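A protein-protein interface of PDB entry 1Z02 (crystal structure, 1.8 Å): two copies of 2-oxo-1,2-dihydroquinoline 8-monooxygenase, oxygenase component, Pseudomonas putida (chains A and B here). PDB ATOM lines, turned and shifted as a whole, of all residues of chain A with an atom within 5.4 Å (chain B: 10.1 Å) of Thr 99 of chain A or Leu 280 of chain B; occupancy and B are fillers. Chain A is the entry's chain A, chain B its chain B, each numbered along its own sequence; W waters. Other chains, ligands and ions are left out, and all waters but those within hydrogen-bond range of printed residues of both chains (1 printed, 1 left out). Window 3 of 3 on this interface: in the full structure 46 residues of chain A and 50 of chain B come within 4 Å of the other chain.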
ATOM      1  N   ARG A  71     -23.713   6.446  -5.785  1.00  0.00           N
ATOM      2  CA  ARG A  71     -23.366   7.860  -5.771  1.00  0.00           C
ATOM      3  C   ARG A  71     -21.859   8.020  -5.687  1.00  0.00           C
ATOM      4  O   ARG A  71     -21.195   7.279  -4.961  1.00  0.00           O
ATOM      5  CB  ARG A  71     -24.002   8.586  -4.578  1.00  0.00           C
ATOM      6  CG  ARG A  71     -23.656  10.080  -4.552  1.00  0.00           C
ATOM      7  CD  ARG A  71     -24.003  10.751  -3.239  1.00  0.00           C
ATOM      8  NE  ARG A  71     -23.652  12.170  -3.273  1.00  0.00           N
ATOM      9  CZ  ARG A  71     -23.517  12.942  -2.196  1.00  0.00           C
ATOM     10  NH1 ARG A  71     -23.198  14.222  -2.331  1.00  0.00           N
ATOM     11  NH2 ARG A  71     -23.688  12.439  -0.980  1.00  0.00           N
ATOM     12  N   CYS A  97     -29.166  14.716  -1.645  1.00  0.00           N
ATOM     13  CA  CYS A  97     -28.073  14.547  -0.686  1.00  0.00           C
ATOM     14  C   CYS A  97     -27.705  15.876  -0.040  1.00  0.00           C
ATOM     15  O   CYS A  97     -27.462  16.870  -0.730  1.00  0.00           O
ATOM     16  CB  CYS A  97     -26.846  13.957  -1.382  1.00  0.00           C
ATOM     17  SG  CYS A  97     -27.156  12.395  -2.257  1.00  0.00           S
ATOM     18  N   PHE A  98     -27.655  15.895   1.289  1.00  0.00           N
ATOM     19  CA  PHE A  98     -27.328  17.124   1.995  1.00  0.00           C
ATOM     20  C   PHE A  98     -25.873  17.242   2.427  1.00  0.00           C
ATOM     21  O   PHE A  98     -25.393  18.345   2.700  1.00  0.00           O
ATOM     22  CB  PHE A  98     -28.255  17.299   3.203  1.00  0.00           C
ATOM     23  CG  PHE A  98     -29.700  17.467   2.828  1.00  0.00           C
ATOM     24  CD1 PHE A  98     -30.572  16.382   2.849  1.00  0.00           C
ATOM     25  CD2 PHE A  98     -30.182  18.707   2.419  1.00  0.00           C
ATOM     26  CE1 PHE A  98     -31.901  16.527   2.461  1.00  0.00           C
ATOM     27  CE2 PHE A  98     -31.513  18.864   2.027  1.00  0.00           C
ATOM     28  CZ  PHE A  98     -32.373  17.770   2.051  1.00  0.00           C
ATOM     29  N   THR A  99     -25.173  16.113   2.491  1.00  0.00           N
ATOM     30  CA  THR A  99     -23.766  16.113   2.880  1.00  0.00           C
ATOM     31  C   THR A  99     -22.985  15.147   2.000  1.00  0.00           C
ATOM     32  O   THR A  99     -23.570  14.384   1.236  1.00  0.00           O
ATOM     33  CB  THR A  99     -23.577  15.712   4.366  1.00  0.00           C
ATOM     34  OG1 THR A  99     -24.050  14.376   4.574  1.00  0.00           O
ATOM     35  CG2 THR A  99     -24.331  16.673   5.277  1.00  0.00           C
ATOM     36  N   LYS A 100     -21.661  15.195   2.116  1.00  0.00           N
ATOM     37  CA  LYS A 100     -20.767  14.347   1.342  1.00  0.00           C
ATOM     38  C   LYS A 100     -20.770  12.885   1.776  1.00  0.00           C
ATOM     39  O   LYS A 100     -20.311  12.019   1.036  1.00  0.00           O
ATOM     40  CB  LYS A 100     -19.336  14.875   1.449  1.00  0.00           C
ATOM     41  CG  LYS A 100     -19.065  16.168   0.698  1.00  0.00           C
ATOM     42  CD  LYS A 100     -19.065  15.938  -0.801  1.00  0.00           C
ATOM     43  CE  LYS A 100     -18.507  17.142  -1.524  1.00  0.00           C
ATOM     44  NZ  LYS A 100     -19.209  18.397  -1.139  1.00  0.00           N
ATOM     45  N   SER A 101     -21.279  12.609   2.971  1.00  0.00           N
ATOM     46  CA  SER A 101     -21.286  11.247   3.482  1.00  0.00           C
ATOM     47  C   SER A 101     -22.657  10.588   3.574  1.00  0.00           C
ATOM     48  O   SER A 101     -22.773   9.491   4.115  1.00  0.00           O
ATOM     49  CB  SER A 101     -20.645  11.231   4.866  1.00  0.00           C
ATOM     50  OG  SER A 101     -21.454  11.945   5.788  1.00  0.00           O
ATOM     51  N   THR A 102     -23.693  11.230   3.048  1.00  0.00           N
ATOM     52  CA  THR A 102     -25.026  10.650   3.145  1.00  0.00           C
ATOM     53  C   THR A 102     -25.853  10.764   1.875  1.00  0.00           C
ATOM     54  O   THR A 102     -25.432  11.361   0.887  1.00  0.00           O
ATOM     55  CB  THR A 102     -25.843  11.332   4.270  1.00  0.00           C
ATOM     56  OG1 THR A 102     -26.101  12.703   3.912  1.00  0.00           O
ATOM     57  CG2 THR A 102     -25.079  11.286   5.584  1.00  0.00           C
ATOM     58  N   SER A 104     -30.273  11.054   1.197  1.00  0.00           N
ATOM     59  CA  SER A 104     -31.561  11.086   1.859  1.00  0.00           C
ATOM     60  C   SER A 104     -32.690  10.658   0.959  1.00  0.00           C
ATOM     61  O   SER A 104     -32.575  10.697  -0.268  1.00  0.00           O
ATOM     62  CB  SER A 104     -31.856  12.492   2.369  1.00  0.00           C
ATOM     63  OG  SER A 104     -30.855  12.921   3.271  1.00  0.00           O
ATOM     64  N   THR A 111     -32.421   9.593   6.292  1.00  0.00           N
ATOM     65  CA  THR A 111     -31.075   9.774   5.756  1.00  0.00           C
ATOM     66  C   THR A 111     -30.124   8.652   6.135  1.00  0.00           C
ATOM     67  O   THR A 111     -30.073   8.222   7.294  1.00  0.00           O
ATOM     68  CB  THR A 111     -30.502  11.127   6.221  1.00  0.00           C
ATOM     69  OG1 THR A 111     -31.428  12.173   5.893  1.00  0.00           O
ATOM     70  CG2 THR A 111     -29.190  11.405   5.537  1.00  0.00           C
ATOM     71  N   VAL A 120     -28.807   7.665   9.904  1.00  0.00           N
ATOM     72  CA  VAL A 120     -28.163   8.674  10.743  1.00  0.00           C
ATOM     73  C   VAL A 120     -29.076   9.789  11.234  1.00  0.00           C
ATOM     74  O   VAL A 120     -28.750  10.483  12.192  1.00  0.00           O
ATOM     75  CB  VAL A 120     -26.958   9.299  10.018  1.00  0.00           C
ATOM     76  CG1 VAL A 120     -25.947   8.213   9.676  1.00  0.00           C
ATOM     77  CG2 VAL A 120     -27.408  10.016   8.767  1.00  0.00           C
ATOM     78  N   THR A 121     -30.223   9.957  10.586  1.00  0.00           N
ATOM     79  CA  THR A 121     -31.169  10.984  10.995  1.00  0.00           C
ATOM     80  C   THR A 121     -32.375  10.964  10.073  1.00  0.00           C
ATOM     81  O   THR A 121     -32.393  10.228   9.092  1.00  0.00           O
ATOM     82  CB  THR A 121     -30.521  12.391  10.933  1.00  0.00           C
ATOM     83  OG1 THR A 121     -31.375  13.358  11.568  1.00  0.00           O
ATOM     84  CG2 THR A 121     -30.288  12.795   9.485  1.00  0.00           C
ATOM     85  N   VAL A 123     -34.701  13.983   8.336  1.00  0.00           N
ATOM     86  CA  VAL A 123     -34.884  15.422   8.183  1.00  0.00           C
ATOM     87  C   VAL A 123     -36.108  15.956   8.924  1.00  0.00           C
ATOM     88  O   VAL A 123     -36.041  16.973   9.604  1.00  0.00           O
ATOM     89  CB  VAL A 123     -34.989  15.818   6.688  1.00  0.00           C
ATOM     90  CG1 VAL A 123     -35.265  17.299   6.565  1.00  0.00           C
ATOM     91  CG2 VAL A 123     -33.686  15.489   5.964  1.00  0.00           C
ATOM     92  N   LEU B 223     -39.525  18.143   1.316  1.00  0.00           N
ATOM     93  CA  LEU B 223     -38.651  17.860   0.183  1.00  0.00           C
ATOM     94  C   LEU B 223     -39.445  17.644  -1.100  1.00  0.00           C
ATOM     95  O   LEU B 223     -38.942  17.880  -2.189  1.00  0.00           O
ATOM     96  CB  LEU B 223     -37.794  16.626   0.470  1.00  0.00           C
ATOM     97  CG  LEU B 223     -36.837  16.739   1.660  1.00  0.00           C
ATOM     98  CD1 LEU B 223     -36.186  15.430   1.906  1.00  0.00           C
ATOM     99  CD2 LEU B 223     -35.785  17.761   1.375  1.00  0.00           C
ATOM    100  N   LEU B 240     -38.706  22.206   8.141  1.00  0.00           N
ATOM    101  CA  LEU B 240     -38.206  20.892   7.769  1.00  0.00           C
ATOM    102  C   LEU B 240     -39.266  19.831   8.042  1.00  0.00           C
ATOM    103  O   LEU B 240     -39.223  18.738   7.476  1.00  0.00           O
ATOM    104  CB  LEU B 240     -36.942  20.563   8.565  1.00  0.00           C
ATOM    105  CG  LEU B 240     -35.717  21.432   8.294  1.00  0.00           C
ATOM    106  CD1 LEU B 240     -34.576  20.955   9.162  1.00  0.00           C
ATOM    107  CD2 LEU B 240     -35.338  21.355   6.821  1.00  0.00           C
ATOM    108  N   GLU B 276     -34.435  22.843  12.221  1.00  0.00           N
ATOM    109  CA  GLU B 276     -33.056  22.465  11.948  1.00  0.00           C
ATOM    110  C   GLU B 276     -32.726  20.986  12.108  1.00  0.00           C
ATOM    111  O   GLU B 276     -33.465  20.222  12.726  1.00  0.00           O
ATOM    112  CB  GLU B 276     -32.110  23.301  12.824  1.00  0.00           C
ATOM    113  CG  GLU B 276     -32.365  23.190  14.320  1.00  0.00           C
ATOM    114  CD  GLU B 276     -31.392  24.020  15.138  1.00  0.00           C
ATOM    115  OE1 GLU B 276     -31.420  23.907  16.376  1.00  0.00           O
ATOM    116  OE2 GLU B 276     -30.601  24.783  14.547  1.00  0.00           O
ATOM    117  N   ASN B 277     -31.602  20.595  11.519  1.00  0.00           N
ATOM    118  CA  ASN B 277     -31.120  19.226  11.597  1.00  0.00           C
ATOM    119  C   ASN B 277     -29.620  19.349  11.841  1.00  0.00           C
ATOM    120  O   ASN B 277     -28.856  19.575  10.908  1.00  0.00           O
ATOM    121  CB  ASN B 277     -31.363  18.483  10.279  1.00  0.00           C
ATOM    122  CG  ASN B 277     -31.140  16.989  10.411  1.00  0.00           C
ATOM    123  OD1 ASN B 277     -32.089  16.213  10.508  1.00  0.00           O
ATOM    124  ND2 ASN B 277     -29.882  16.582  10.432  1.00  0.00           N
ATOM    125  N   GLN B 278     -29.205  19.204  13.091  1.00  0.00           N
ATOM    126  CA  GLN B 278     -27.802  19.334  13.449  1.00  0.00           C
ATOM    127  C   GLN B 278     -26.890  18.341  12.750  1.00  0.00           C
ATOM    128  O   GLN B 278     -25.780  18.688  12.357  1.00  0.00           O
ATOM    129  CB  GLN B 278     -27.664  19.226  14.971  1.00  0.00           C
ATOM    130  CG  GLN B 278     -28.176  20.466  15.699  1.00  0.00           C
ATOM    131  CD  GLN B 278     -28.232  20.296  17.193  1.00  0.00           C
ATOM    132  OE1 GLN B 278     -27.483  19.514  17.769  1.00  0.00           O
ATOM    133  NE2 GLN B 278     -29.116  21.039  17.834  1.00  0.00           N
ATOM    134  N   GLU B 279     -27.358  17.111  12.577  1.00  0.00           N
ATOM    135  CA  GLU B 279     -26.562  16.069  11.928  1.00  0.00           C
ATOM    136  C   GLU B 279     -26.122  16.426  10.509  1.00  0.00           C
ATOM    137  O   GLU B 279     -24.980  16.187  10.115  1.00  0.00           O
ATOM    138  CB  GLU B 279     -27.358  14.762  11.894  1.00  0.00           C
ATOM    139  CG  GLU B 279     -26.608  13.581  11.296  1.00  0.00           C
ATOM    140  CD  GLU B 279     -25.335  13.253  12.054  1.00  0.00           C
ATOM    141  OE1 GLU B 279     -25.326  13.414  13.292  1.00  0.00           O
ATOM    142  OE2 GLU B 279     -24.350  12.821  11.414  1.00  0.00           O
ATOM    143  N   LEU B 280     -27.039  17.008   9.748  1.00  0.00           N
ATOM    144  CA  LEU B 280     -26.775  17.378   8.363  1.00  0.00           C
ATOM    145  C   LEU B 280     -26.363  18.838   8.213  1.00  0.00           C
ATOM    146  O   LEU B 280     -25.951  19.264   7.135  1.00  0.00           O
ATOM    147  CB  LEU B 280     -28.024  17.109   7.515  1.00  0.00           C
ATOM    148  CG  LEU B 280     -28.532  15.661   7.538  1.00  0.00           C
ATOM    149  CD1 LEU B 280     -29.852  15.544   6.803  1.00  0.00           C
ATOM    150  CD2 LEU B 280     -27.505  14.768   6.886  1.00  0.00           C
ATOM    151  N   GLY B 281     -26.480  19.606   9.289  1.00  0.00           N
ATOM    152  CA  GLY B 281     -26.120  21.008   9.219  1.00  0.00           C
ATOM    153  C   GLY B 281     -27.184  21.833   8.511  1.00  0.00           C
ATOM    154  O   GLY B 281     -26.868  22.787   7.797  1.00  0.00           O
ATOM    155  N   LEU B 282     -28.447  21.466   8.698  1.00  0.00           N
ATOM    156  CA  LEU B 282     -29.546  22.194   8.076  1.00  0.00           C
ATOM    157  C   LEU B 282     -30.170  23.142   9.085  1.00  0.00           C
ATOM    158  O   LEU B 282     -30.241  22.841  10.279  1.00  0.00           O
ATOM    159  CB  LEU B 282     -30.617  21.236   7.566  1.00  0.00           C
ATOM    160  CG  LEU B 282     -30.188  20.224   6.511  1.00  0.00           C
ATOM    161  CD1 LEU B 282     -31.427  19.502   6.034  1.00  0.00           C
ATOM    162  CD2 LEU B 282     -29.478  20.909   5.351  1.00  0.00           C
ATOM    163  N   LYS B 283     -30.650  24.278   8.596  1.00  0.00           N
ATOM    164  CA  LYS B 283     -31.227  25.260   9.482  1.00  0.00           C
ATOM    165  C   LYS B 283     -32.087  26.278   8.752  1.00  0.00           C
ATOM    166  O   LYS B 283     -31.621  26.950   7.839  1.00  0.00           O
ATOM    167  CB  LYS B 283     -30.096  25.962  10.208  1.00  0.00           C
ATOM    168  CG  LYS B 283     -30.537  27.038  11.120  1.00  0.00           C
ATOM    169  CD  LYS B 283     -29.341  27.537  11.838  1.00  0.00           C
ATOM    170  CE  LYS B 283     -29.749  28.401  12.986  1.00  0.00           C
ATOM    171  NZ  LYS B 283     -28.546  28.771  13.760  1.00  0.00           N
HETATM  172  O   HOH W   1     -26.220  20.416   4.449  1.00  0.00           O
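No residue of chain B comes within 4 Å of Cys 97 of chain A. Of chain B, only Leu 280 (3.6 Å) comes within 4 Å of Thr 99 of chain A. No residue of chain B comes within 4 Å of Ser 101 of chain A. Thr 102 of chain A touches just one residue of chain B: Leu 280 (3.9 Å). Of the printed residues of chain B, Thr 111 of chain A touches Leu 280. Of the printed residues of chain B, Val 120 of chain A touches Glu 279. Of the printed residues of chain B, Thr 121 of chain A touches Asn 277 and Leu 280. Printed residues of chain B within 4 Å of Val 123 of chain A: Leu 240 (3.8 Å), Asn 277 (3.7 Å) and Leu 280 (3.9 Å). Gln 278 of chain B touches none of the printed residues of chain A. Printed residues of chain A within 4 Å of Glu 279 of chain B: Val 120. Leu 280 of chain B touches five residues of chain A. Lys 283 of chain B touches none of the printed residues of chain A. The nearest residue of chain A that does not touch Leu 280 of chain B is Phe 98 of chain A (4.1 Å).
Among the printed residues, pairs that only touch across the chains: Phe 98 of chain A with Leu 223 of chain B (3.5 Å), Phe 98 of chain A with Leu 282 of chain B (3.7 Å), Thr 99 of chain A with Leu 280 of chain B (3.6 Å), Thr 102 of chain A with Leu 280 of chain B (3.9 Å), Thr 111 of chain A with Leu 280 of chain B (3.8 Å), Val 120 of chain A with Glu 279 of chain B (3.9 Å), Thr 121 of chain A with Leu 280 of chain B (3.9 Å), Val 123 of chain A with Leu 240 of chain B (3.8 Å), Val 123 of chain A with Asn 277 of chain B (3.7 Å) and Val 123 of chain A with Leu 280 of chain B (3.9 Å).
Of the 12 printed residues of chain A, 7 touch a printed residue of chain B. Hydrophobic or aromatic side chains of chain A that line the printed part of chain B: Phe 98 and Val 123. Along chain A the printed residues that touch a printed residue of chain B span positions 98 to 123. Among the printed residues, no Asp or Glu carboxylate lies within 4 Å of a Lys or Arg side-chain nitrogen of the other chain.
No position is printed for both chains. Of the 11 pairs that touch across the chains among the printed residues, none has its exchanged pair printed and touching as well.
NH2 of Arg 71 of chain A sits at hydrogen-bond distance from O of Thr 99 of chain A, at 3.0 Å. NH2 of Arg 71 of chain A lies within hydrogen-bond range of O of Thr 102 of chain A (2.8 Å). The side-chain sulfur of Cys 97 of chain A sits close to the backbone carbonyl oxygen of Thr 102 of chain A (3.7 Å). The side-chain hydroxyl (OG) of Ser 104 of chain A lies within hydrogen-bond range of the side-chain hydroxyl (OG1) of Thr 111 of chain A. The backbone carbonyl oxygen (O) of Thr 121 of chain A lies within hydrogen-bond range of the backbone NH (N) of Thr 111 of chain A, at 2.9 Å. ND2 of Asn 277 of chain B sits close to N of Glu 279 of chain B.
The side-chain amide oxygen (OD1) of Asn 277 of chain B is in hydrogen-bond range of the side-chain hydroxyl (OG1) of Thr 121 of chain A (3.1 Å).
Water W1 lies within hydrogen-bond range of the backbone carbonyl oxygen of Phe 98 of chain A and the backbone carbonyl oxygen of Leu 280 of chain B.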
